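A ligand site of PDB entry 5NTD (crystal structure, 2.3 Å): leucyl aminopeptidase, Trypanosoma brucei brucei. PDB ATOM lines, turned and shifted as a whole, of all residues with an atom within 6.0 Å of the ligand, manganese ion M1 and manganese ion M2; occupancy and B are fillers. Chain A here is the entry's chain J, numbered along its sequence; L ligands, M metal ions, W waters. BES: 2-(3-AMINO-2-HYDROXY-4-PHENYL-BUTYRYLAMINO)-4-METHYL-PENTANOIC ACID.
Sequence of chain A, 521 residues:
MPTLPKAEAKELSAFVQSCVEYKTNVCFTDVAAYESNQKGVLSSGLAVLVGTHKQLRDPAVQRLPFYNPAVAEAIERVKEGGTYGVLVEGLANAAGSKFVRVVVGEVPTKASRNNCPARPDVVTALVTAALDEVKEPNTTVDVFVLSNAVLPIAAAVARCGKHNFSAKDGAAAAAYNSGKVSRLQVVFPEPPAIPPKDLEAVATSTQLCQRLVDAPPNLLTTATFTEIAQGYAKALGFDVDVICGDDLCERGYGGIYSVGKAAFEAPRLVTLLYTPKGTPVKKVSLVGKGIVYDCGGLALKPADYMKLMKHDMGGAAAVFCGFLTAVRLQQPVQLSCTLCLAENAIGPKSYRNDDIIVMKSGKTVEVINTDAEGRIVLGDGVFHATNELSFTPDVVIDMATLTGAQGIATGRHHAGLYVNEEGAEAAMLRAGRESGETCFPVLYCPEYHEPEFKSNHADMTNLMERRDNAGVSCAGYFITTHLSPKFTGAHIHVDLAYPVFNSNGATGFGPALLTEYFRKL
O4 of the ligand sits at hydrogen-bond distance from N of Gly 404 (3.0 Å).
The side-chain amino group (NZ) of Lys 301 sits close to an oxygen (O3) of the ligand (2.8 Å).
The backbone carbonyl oxygen of Thr 401 sits close to a nitrogen (N2) of the ligand, at 3.2 Å.
NH2 of Arg 467 is in salt-bridge range of O1 of the ligand, at 3.2 Å.
The backbone NH (N) of Asp 371 sits at hydrogen-bond distance from the backbone carbonyl oxygen (O) of Gly 296, 3.2 Å away.
The side-chain amide nitrogen (ND2) of Asn 344 is in hydrogen-bond range of the side-chain carboxylate (OD1) of Asp 294 (3.0 Å).
The backbone NH (N) of Asp 371 sits at hydrogen-bond distance from the side-chain amide oxygen (OD1) of Asn 369 (2.7 Å).
The backbone carbonyl oxygen of Asp 312 sits at hydrogen-bond distance from the backbone NH of Ile 291 (3.3 Å).
The side-chain amide nitrogen (ND2) of Asn 344 sits close to the side-chain carboxylate (OE2) of Glu 373.
The side-chain amino group of Lys 289 lies close to the backbone carbonyl oxygen of Thr 401.
The side-chain amino group of Lys 301 is in salt-bridge range of the side-chain carboxylate of Asp 371 (2.7 Å).
The side-chain carboxylate of Asp 294 lies within hydrogen-bond range of the backbone NH of Gly 296 (3.2 Å).
Met 309 touches the ligand.
CG of Asn 369 touches C16 of the ligand, at 3.7 Å.
O of Leu 402 touches C6 of the ligand, at 3.3 Å.
Thr 403 touches the ligand.
Leu 463 touches the ligand (CD1 to C16, 3.6 Å).
CB of Ala 497 touches C8 of the ligand (3.8 Å).
Tyr 498 touches the ligand (OH to C11, 3.8 Å).
Hydrophobic or aromatic side chains that line the ligand: Met 309, Leu 463, Ala 497 and Tyr 498.
Along chain A the residues within 4 Å of the ligand span positions 289 to 498.
The nearest printed residue that does not touch the ligand is Ala 372 (4.002 Å).
NZ of Lys 301 touches manganese ion M1, 3.9 Å away.
Four residues have an atom within 4 Å of manganese ion M2: Lys 289, Asp 294, Asp 312 and Glu 373.
Manganese ion M1 is bound by an oxygen (O2) of the ligand (2.0 Å), the side-chain carboxylate of Asp 371 (2.0 Å), the backbone carbonyl oxygen of Asp 371 (2.0 Å), the side-chain carboxylate of Glu 373 (2.0 Å), an oxygen (O3) of the ligand (2.0 Å) and the side-chain carboxylate of Asp 294 (2.0 Å).
Manganese ion M2 is bound by an oxygen (O2) of the ligand (1.9 Å), the side-chain carboxylate of Glu 373 (1.9 Å), the side-chain carboxylate of Asp 312 (2.0 Å), the side-chain amino group of Lys 289 (2.0 Å), the side-chain carboxylate of Asp 294 (2.0 Å) and a nitrogen (N2) of the ligand (2.0 Å).
Manganese ion M2 has six donor atoms within binding distance.
Water W1 lies within hydrogen-bond range of OD1 of Asp 312 and SD of Met 309.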
ATOM      1  N   LYS A 289       7.782 -17.184 -27.369  1.00  0.00           N
ATOM      2  CA  LYS A 289       6.678 -18.148 -27.117  1.00  0.00           C
ATOM      3  C   LYS A 289       6.464 -18.904 -28.401  1.00  0.00           C
ATOM      4  O   LYS A 289       6.052 -18.344 -29.388  1.00  0.00           O
ATOM      5  CB  LYS A 289       5.370 -17.493 -26.668  1.00  0.00           C
ATOM      6  CG  LYS A 289       4.198 -18.460 -26.487  1.00  0.00           C
ATOM      7  CD  LYS A 289       2.843 -17.764 -26.223  1.00  0.00           C
ATOM      8  CE  LYS A 289       1.669 -18.736 -26.136  1.00  0.00           C
ATOM      9  NZ  LYS A 289       0.262 -18.211 -25.903  1.00  0.00           N
ATOM     10  N   ILE A 291       4.520 -21.693 -29.127  1.00  0.00           N
ATOM     11  CA  ILE A 291       3.413 -22.631 -28.999  1.00  0.00           C
ATOM     12  C   ILE A 291       2.898 -22.886 -30.409  1.00  0.00           C
ATOM     13  O   ILE A 291       2.162 -22.105 -30.985  1.00  0.00           O
ATOM     14  CB  ILE A 291       2.323 -22.156 -28.059  1.00  0.00           C
ATOM     15  CG1 ILE A 291       2.911 -21.977 -26.653  1.00  0.00           C
ATOM     16  CG2 ILE A 291       1.160 -23.143 -28.033  1.00  0.00           C
ATOM     17  CD1 ILE A 291       3.485 -23.223 -26.015  1.00  0.00           C
ATOM     18  N   ASP A 294      -2.051 -24.004 -29.846  1.00  0.00           N
ATOM     19  CA  ASP A 294      -2.637 -23.766 -28.524  1.00  0.00           C
ATOM     20  C   ASP A 294      -4.087 -24.263 -28.591  1.00  0.00           C
ATOM     21  O   ASP A 294      -4.985 -23.501 -28.909  1.00  0.00           O
ATOM     22  CB  ASP A 294      -2.558 -22.264 -28.107  1.00  0.00           C
ATOM     23  CG  ASP A 294      -2.881 -22.006 -26.602  1.00  0.00           C
ATOM     24  OD1 ASP A 294      -3.168 -23.022 -25.944  1.00  0.00           O
ATOM     25  OD2 ASP A 294      -2.804 -20.784 -26.084  1.00  0.00           O
ATOM     26  N   GLY A 296      -5.582 -25.053 -25.907  1.00  0.00           N
ATOM     27  CA  GLY A 296      -6.020 -24.713 -24.534  1.00  0.00           C
ATOM     28  C   GLY A 296      -5.624 -25.728 -23.457  1.00  0.00           C
ATOM     29  O   GLY A 296      -5.665 -25.463 -22.271  1.00  0.00           O
ATOM     30  N   LYS A 301     -10.168 -24.700 -25.626  1.00  0.00           N
ATOM     31  CA  LYS A 301     -10.754 -23.575 -26.349  1.00  0.00           C
ATOM     32  C   LYS A 301     -11.946 -24.023 -27.174  1.00  0.00           C
ATOM     33  O   LYS A 301     -11.906 -25.094 -27.779  1.00  0.00           O
ATOM     34  CB  LYS A 301      -9.777 -22.900 -27.299  1.00  0.00           C
ATOM     35  CG  LYS A 301      -8.605 -22.288 -26.621  1.00  0.00           C
ATOM     36  CD  LYS A 301      -7.721 -21.612 -27.657  1.00  0.00           C
ATOM     37  CE  LYS A 301      -6.493 -21.053 -27.009  1.00  0.00           C
ATOM     38  NZ  LYS A 301      -6.838 -19.937 -26.100  1.00  0.00           N
ATOM     39  N   MET A 309      -4.785 -20.474 -33.816  1.00  0.00           N
ATOM     40  CA  MET A 309      -3.770 -20.723 -32.768  1.00  0.00           C
ATOM     41  C   MET A 309      -2.477 -21.359 -33.322  1.00  0.00           C
ATOM     42  O   MET A 309      -1.524 -21.570 -32.607  1.00  0.00           O
ATOM     43  CB  MET A 309      -4.344 -21.507 -31.577  1.00  0.00           C
ATOM     44  CG  MET A 309      -5.358 -20.711 -30.778  1.00  0.00           C
ATOM     45  SD  MET A 309      -4.609 -19.242 -30.012  1.00  0.00           S
ATOM     46  CE  MET A 309      -5.833 -17.989 -30.340  1.00  0.00           C
ATOM     47  N   ASP A 312       0.287 -19.074 -32.688  1.00  0.00           N
ATOM     48  CA  ASP A 312       0.716 -18.959 -31.278  1.00  0.00           C
ATOM     49  C   ASP A 312       2.232 -19.126 -31.099  1.00  0.00           C
ATOM     50  O   ASP A 312       2.753 -19.066 -29.998  1.00  0.00           O
ATOM     51  CB  ASP A 312      -0.064 -19.897 -30.335  1.00  0.00           C
ATOM     52  CG  ASP A 312      -0.309 -19.293 -28.980  1.00  0.00           C
ATOM     53  OD1 ASP A 312      -0.370 -18.031 -28.915  1.00  0.00           O
ATOM     54  OD2 ASP A 312      -0.519 -20.005 -27.946  1.00  0.00           O
ATOM     55  N   ASN A 344       0.487 -27.152 -26.955  1.00  0.00           N
ATOM     56  CA  ASN A 344      -0.442 -27.237 -25.825  1.00  0.00           C
ATOM     57  C   ASN A 344      -1.599 -28.143 -26.252  1.00  0.00           C
ATOM     58  O   ASN A 344      -2.568 -27.710 -26.860  1.00  0.00           O
ATOM     59  CB  ASN A 344      -0.936 -25.877 -25.381  1.00  0.00           C
ATOM     60  CG  ASN A 344      -1.568 -25.900 -23.990  1.00  0.00           C
ATOM     61  OD1 ASN A 344      -1.412 -26.821 -23.231  1.00  0.00           O
ATOM     62  ND2 ASN A 344      -2.319 -24.847 -23.679  1.00  0.00           N
ATOM     63  N   ASN A 369      -5.496 -22.563 -14.776  1.00  0.00           N
ATOM     64  CA  ASN A 369      -6.001 -22.702 -16.144  1.00  0.00           C
ATOM     65  C   ASN A 369      -4.870 -23.063 -17.101  1.00  0.00           C
ATOM     66  O   ASN A 369      -3.948 -22.293 -17.315  1.00  0.00           O
ATOM     67  CB  ASN A 369      -6.694 -21.418 -16.584  1.00  0.00           C
ATOM     68  CG  ASN A 369      -7.493 -21.571 -17.849  1.00  0.00           C
ATOM     69  OD1 ASN A 369      -6.959 -21.999 -18.868  1.00  0.00           O
ATOM     70  ND2 ASN A 369      -8.753 -21.192 -17.815  1.00  0.00           N
ATOM     71  N   THR A 370      -5.015 -24.212 -17.733  1.00  0.00           N
ATOM     72  CA  THR A 370      -3.982 -24.743 -18.667  1.00  0.00           C
ATOM     73  C   THR A 370      -3.859 -23.951 -19.955  1.00  0.00           C
ATOM     74  O   THR A 370      -2.873 -24.085 -20.664  1.00  0.00           O
ATOM     75  CB  THR A 370      -4.241 -26.196 -19.060  1.00  0.00           C
ATOM     76  OG1 THR A 370      -5.543 -26.297 -19.688  1.00  0.00           O
ATOM     77  CG2 THR A 370      -4.178 -27.105 -17.848  1.00  0.00           C
ATOM     78  N   ASP A 371      -4.858 -23.110 -20.247  1.00  0.00           N
ATOM     79  CA  ASP A 371      -4.837 -22.252 -21.430  1.00  0.00           C
ATOM     80  C   ASP A 371      -4.012 -20.972 -21.275  1.00  0.00           C
ATOM     81  O   ASP A 371      -3.767 -20.234 -22.281  1.00  0.00           O
ATOM     82  CB  ASP A 371      -6.212 -21.928 -21.906  1.00  0.00           C
ATOM     83  CG  ASP A 371      -6.243 -21.456 -23.355  1.00  0.00           C
ATOM     84  OD1 ASP A 371      -5.203 -21.511 -24.091  1.00  0.00           O
ATOM     85  OD2 ASP A 371      -7.342 -20.970 -23.703  1.00  0.00           O
ATOM     86  N   ALA A 372      -3.583 -20.742 -20.047  1.00  0.00           N
ATOM     87  CA  ALA A 372      -2.537 -19.721 -19.722  1.00  0.00           C
ATOM     88  C   ALA A 372      -1.133 -20.386 -19.678  1.00  0.00           C
ATOM     89  O   ALA A 372      -0.450 -20.375 -18.668  1.00  0.00           O
ATOM     90  CB  ALA A 372      -2.849 -18.987 -18.423  1.00  0.00           C
ATOM     91  N   GLU A 373      -0.785 -20.976 -20.803  1.00  0.00           N
ATOM     92  CA  GLU A 373       0.408 -21.826 -20.954  1.00  0.00           C
ATOM     93  C   GLU A 373       1.631 -21.018 -21.302  1.00  0.00           C
ATOM     94  O   GLU A 373       2.744 -21.370 -20.986  1.00  0.00           O
ATOM     95  CB  GLU A 373       0.162 -22.873 -22.035  1.00  0.00           C
ATOM     96  CG  GLU A 373       0.338 -22.460 -23.521  1.00  0.00           C
ATOM     97  CD  GLU A 373      -0.690 -21.487 -24.103  1.00  0.00           C
ATOM     98  OE1 GLU A 373      -0.335 -20.776 -25.130  1.00  0.00           O
ATOM     99  OE2 GLU A 373      -1.862 -21.431 -23.604  1.00  0.00           O
ATOM    100  N   GLY A 374       1.397 -19.930 -22.012  1.00  0.00           N
ATOM    101  CA  GLY A 374       2.487 -19.128 -22.589  1.00  0.00           C
ATOM    102  C   GLY A 374       3.387 -18.546 -21.543  1.00  0.00           C
ATOM    103  O   GLY A 374       4.592 -18.626 -21.614  1.00  0.00           O
ATOM    104  N   ARG A 375       2.763 -18.009 -20.524  1.00  0.00           N
ATOM    105  CA  ARG A 375       3.528 -17.368 -19.437  1.00  0.00           C
ATOM    106  C   ARG A 375       4.416 -18.395 -18.710  1.00  0.00           C
ATOM    107  O   ARG A 375       5.450 -18.074 -18.203  1.00  0.00           O
ATOM    108  CB  ARG A 375       2.605 -16.609 -18.480  1.00  0.00           C
ATOM    109  CG  ARG A 375       1.729 -17.489 -17.629  1.00  0.00           C
ATOM    110  CD  ARG A 375       0.612 -16.714 -17.002  1.00  0.00           C
ATOM    111  NE  ARG A 375      -0.349 -16.283 -17.997  1.00  0.00           N
ATOM    112  CZ  ARG A 375      -1.299 -15.375 -17.783  1.00  0.00           C
ATOM    113  NH1 ARG A 375      -1.446 -14.824 -16.577  1.00  0.00           N
ATOM    114  NH2 ARG A 375      -2.118 -15.032 -18.764  1.00  0.00           N
ATOM    115  N   THR A 401       2.680 -14.201 -28.288  1.00  0.00           N
ATOM    116  CA  THR A 401       1.248 -14.012 -28.612  1.00  0.00           C
ATOM    117  C   THR A 401       0.457 -14.385 -27.379  1.00  0.00           C
ATOM    118  O   THR A 401      -0.188 -15.420 -27.324  1.00  0.00           O
ATOM    119  CB  THR A 401       0.837 -14.884 -29.825  1.00  0.00           C
ATOM    120  OG1 THR A 401       1.327 -16.207 -29.619  1.00  0.00           O
ATOM    121  CG2 THR A 401       1.433 -14.305 -31.095  1.00  0.00           C
ATOM    122  N   LEU A 402       0.513 -13.529 -26.391  1.00  0.00           N
ATOM    123  CA  LEU A 402       0.233 -13.965 -25.024  1.00  0.00           C
ATOM    124  C   LEU A 402      -1.207 -13.837 -24.530  1.00  0.00           C
ATOM    125  O   LEU A 402      -1.688 -14.729 -23.844  1.00  0.00           O
ATOM    126  CB  LEU A 402       1.179 -13.314 -24.056  1.00  0.00           C
ATOM    127  CG  LEU A 402       1.309 -14.054 -22.707  1.00  0.00           C
ATOM    128  CD1 LEU A 402       1.802 -15.501 -22.896  1.00  0.00           C
ATOM    129  CD2 LEU A 402       2.278 -13.312 -21.817  1.00  0.00           C
ATOM    130  N   THR A 403      -1.876 -12.728 -24.831  1.00  0.00           N
ATOM    131  CA  THR A 403      -3.211 -12.466 -24.245  1.00  0.00           C
ATOM    132  C   THR A 403      -4.190 -11.857 -25.221  1.00  0.00           C
ATOM    133  O   THR A 403      -3.843 -11.041 -26.063  1.00  0.00           O
ATOM    134  CB  THR A 403      -3.146 -11.481 -23.062  1.00  0.00           C
ATOM    135  OG1 THR A 403      -2.753 -10.184 -23.512  1.00  0.00           O
ATOM    136  CG2 THR A 403      -2.197 -11.944 -21.990  1.00  0.00           C
ATOM    137  N   GLY A 404      -5.437 -12.251 -25.070  1.00  0.00           N
ATOM    138  CA  GLY A 404      -6.541 -11.605 -25.773  1.00  0.00           C
ATOM    139  C   GLY A 404      -6.722 -10.176 -25.306  1.00  0.00           C
ATOM    140  O   GLY A 404      -7.085  -9.306 -26.049  1.00  0.00           O
ATOM    141  N   ALA A 405      -6.403  -9.962 -24.051  1.00  0.00           N
ATOM    142  CA  ALA A 405      -6.374  -8.629 -23.469  1.00  0.00           C
ATOM    143  C   ALA A 405      -5.546  -7.638 -24.307  1.00  0.00           C
ATOM    144  O   ALA A 405      -5.842  -6.454 -24.359  1.00  0.00           O
ATOM    145  CB  ALA A 405      -5.850  -8.681 -22.040  1.00  0.00           C
ATOM    146  N   LEU A 463      -2.752 -17.681 -13.075  1.00  0.00           N
ATOM    147  CA  LEU A 463      -3.880 -16.875 -13.553  1.00  0.00           C
ATOM    148  C   LEU A 463      -4.396 -15.949 -12.486  1.00  0.00           C
ATOM    149  O   LEU A 463      -4.532 -16.327 -11.352  1.00  0.00           O
ATOM    150  CB  LEU A 463      -5.000 -17.747 -14.062  1.00  0.00           C
ATOM    151  CG  LEU A 463      -6.113 -17.020 -14.807  1.00  0.00           C
ATOM    152  CD1 LEU A 463      -5.638 -16.564 -16.164  1.00  0.00           C
ATOM    153  CD2 LEU A 463      -7.342 -17.891 -14.990  1.00  0.00           C
ATOM    154  N   ARG A 467      -9.681 -11.002 -13.525  1.00  0.00           N
ATOM    155  CA  ARG A 467      -9.199 -10.875 -14.907  1.00  0.00           C
ATOM    156  C   ARG A 467      -9.363  -9.472 -15.494  1.00  0.00           C
ATOM    157  O   ARG A 467      -8.828  -9.151 -16.568  1.00  0.00           O
ATOM    158  CB  ARG A 467      -9.826 -11.927 -15.782  1.00  0.00           C
ATOM    159  CG  ARG A 467      -9.501 -13.334 -15.265  1.00  0.00           C
ATOM    160  CD  ARG A 467      -8.601 -14.136 -16.159  1.00  0.00           C
ATOM    161  NE  ARG A 467      -8.999 -14.023 -17.575  1.00  0.00           N
ATOM    162  CZ  ARG A 467      -8.179 -13.896 -18.619  1.00  0.00           C
ATOM    163  NH1 ARG A 467      -6.853 -13.851 -18.471  1.00  0.00           N
ATOM    164  NH2 ARG A 467      -8.716 -13.832 -19.847  1.00  0.00           N
ATOM    165  N   ALA A 497       0.068 -10.632 -29.605  1.00  0.00           N
ATOM    166  CA  ALA A 497      -1.040 -11.577 -29.936  1.00  0.00           C
ATOM    167  C   ALA A 497      -1.717 -11.243 -31.280  1.00  0.00           C
ATOM    168  O   ALA A 497      -1.898 -12.089 -32.121  1.00  0.00           O
ATOM    169  CB  ALA A 497      -2.078 -11.595 -28.829  1.00  0.00           C
ATOM    170  N   TYR A 498      -2.071  -9.986 -31.456  1.00  0.00           N
ATOM    171  CA  TYR A 498      -2.788  -9.548 -32.688  1.00  0.00           C
ATOM    172  C   TYR A 498      -1.923  -8.992 -33.836  1.00  0.00           C
ATOM    173  O   TYR A 498      -2.243  -9.215 -34.982  1.00  0.00           O
ATOM    174  CB  TYR A 498      -3.908  -8.587 -32.329  1.00  0.00           C
ATOM    175  CG  TYR A 498      -5.032  -9.280 -31.633  1.00  0.00           C
ATOM    176  CD1 TYR A 498      -5.010  -9.495 -30.269  1.00  0.00           C
ATOM    177  CD2 TYR A 498      -6.134  -9.757 -32.357  1.00  0.00           C
ATOM    178  CE1 TYR A 498      -6.047 -10.139 -29.632  1.00  0.00           C
ATOM    179  CE2 TYR A 498      -7.175 -10.424 -31.726  1.00  0.00           C
ATOM    180  CZ  TYR A 498      -7.128 -10.615 -30.375  1.00  0.00           C
ATOM    181  OH  TYR A 498      -8.158 -11.270 -29.732  1.00  0.00           O
ATOM    182  N   PHE A 501      -0.787 -11.070 -37.150  1.00  0.00           N
ATOM    183  CA  PHE A 501      -1.685 -11.483 -38.217  1.00  0.00           C
ATOM    184  C   PHE A 501      -2.705 -10.439 -38.612  1.00  0.00           C
ATOM    185  O   PHE A 501      -3.014  -9.524 -37.881  1.00  0.00           O
ATOM    186  CB  PHE A 501      -2.382 -12.830 -37.850  1.00  0.00           C
ATOM    187  CG  PHE A 501      -3.552 -12.680 -36.914  1.00  0.00           C
ATOM    188  CD1 PHE A 501      -3.346 -12.633 -35.558  1.00  0.00           C
ATOM    189  CD2 PHE A 501      -4.851 -12.605 -37.388  1.00  0.00           C
ATOM    190  CE1 PHE A 501      -4.410 -12.479 -34.684  1.00  0.00           C
ATOM    191  CE2 PHE A 501      -5.916 -12.463 -36.536  1.00  0.00           C
ATOM    192  CZ  PHE A 501      -5.691 -12.409 -35.171  1.00  0.00           C
HETATM  193  N2  BES L   1      -2.279 -17.879 -27.020  1.00  0.00           N
HETATM  194  C1  BES L   1      -3.337 -17.271 -26.226  1.00  0.00           C
HETATM  195  C6  BES L   1      -3.456 -15.736 -26.386  1.00  0.00           C
HETATM  196  C7  BES L   1      -4.221 -15.237 -27.620  1.00  0.00           C
HETATM  197  C8  BES L   1      -3.586 -15.062 -28.851  1.00  0.00           C
HETATM  198  C12 BES L   1      -5.593 -14.914 -27.565  1.00  0.00           C
HETATM  199  C9  BES L   1      -4.288 -14.579 -29.992  1.00  0.00           C
HETATM  200  C11 BES L   1      -6.304 -14.449 -28.697  1.00  0.00           C
HETATM  201  C10 BES L   1      -5.669 -14.274 -29.927  1.00  0.00           C
HETATM  202  C2  BES L   1      -3.110 -17.716 -24.776  1.00  0.00           C
HETATM  203  O2  BES L   1      -2.365 -19.000 -24.699  1.00  0.00           O
HETATM  204  C3  BES L   1      -4.459 -17.943 -24.153  1.00  0.00           C
HETATM  205  O3  BES L   1      -4.911 -19.087 -24.256  1.00  0.00           O
HETATM  206  N1  BES L   1      -4.915 -16.870 -23.486  1.00  0.00           N
HETATM  207  C4  BES L   1      -6.127 -16.794 -22.721  1.00  0.00           C
HETATM  208  C13 BES L   1      -5.896 -17.165 -21.250  1.00  0.00           C
HETATM  209  C14 BES L   1      -7.149 -17.465 -20.404  1.00  0.00           C
HETATM  210  C15 BES L   1      -8.275 -18.294 -21.036  1.00  0.00           C
HETATM  211  C16 BES L   1      -6.700 -18.173 -19.149  1.00  0.00           C
HETATM  212  C5  BES L   1      -6.665 -15.396 -22.828  1.00  0.00           C
HETATM  213  O1  BES L   1      -7.883 -15.244 -22.652  1.00  0.00           O
HETATM  214  O4  BES L   1      -5.914 -14.458 -23.129  1.00  0.00           O
HETATM  215 MN    MN M   1      -3.510 -20.517 -24.221  1.00  0.00          MN
HETATM  216 MN    MN M   2      -1.272 -19.466 -26.216  1.00  0.00          MN
HETATM  217  O   HOH W   1      -2.039 -17.197 -31.117  1.00  0.00           O
HETATM  218  O   HOH W   2      -6.698 -12.212 -21.908  1.00  0.00           O
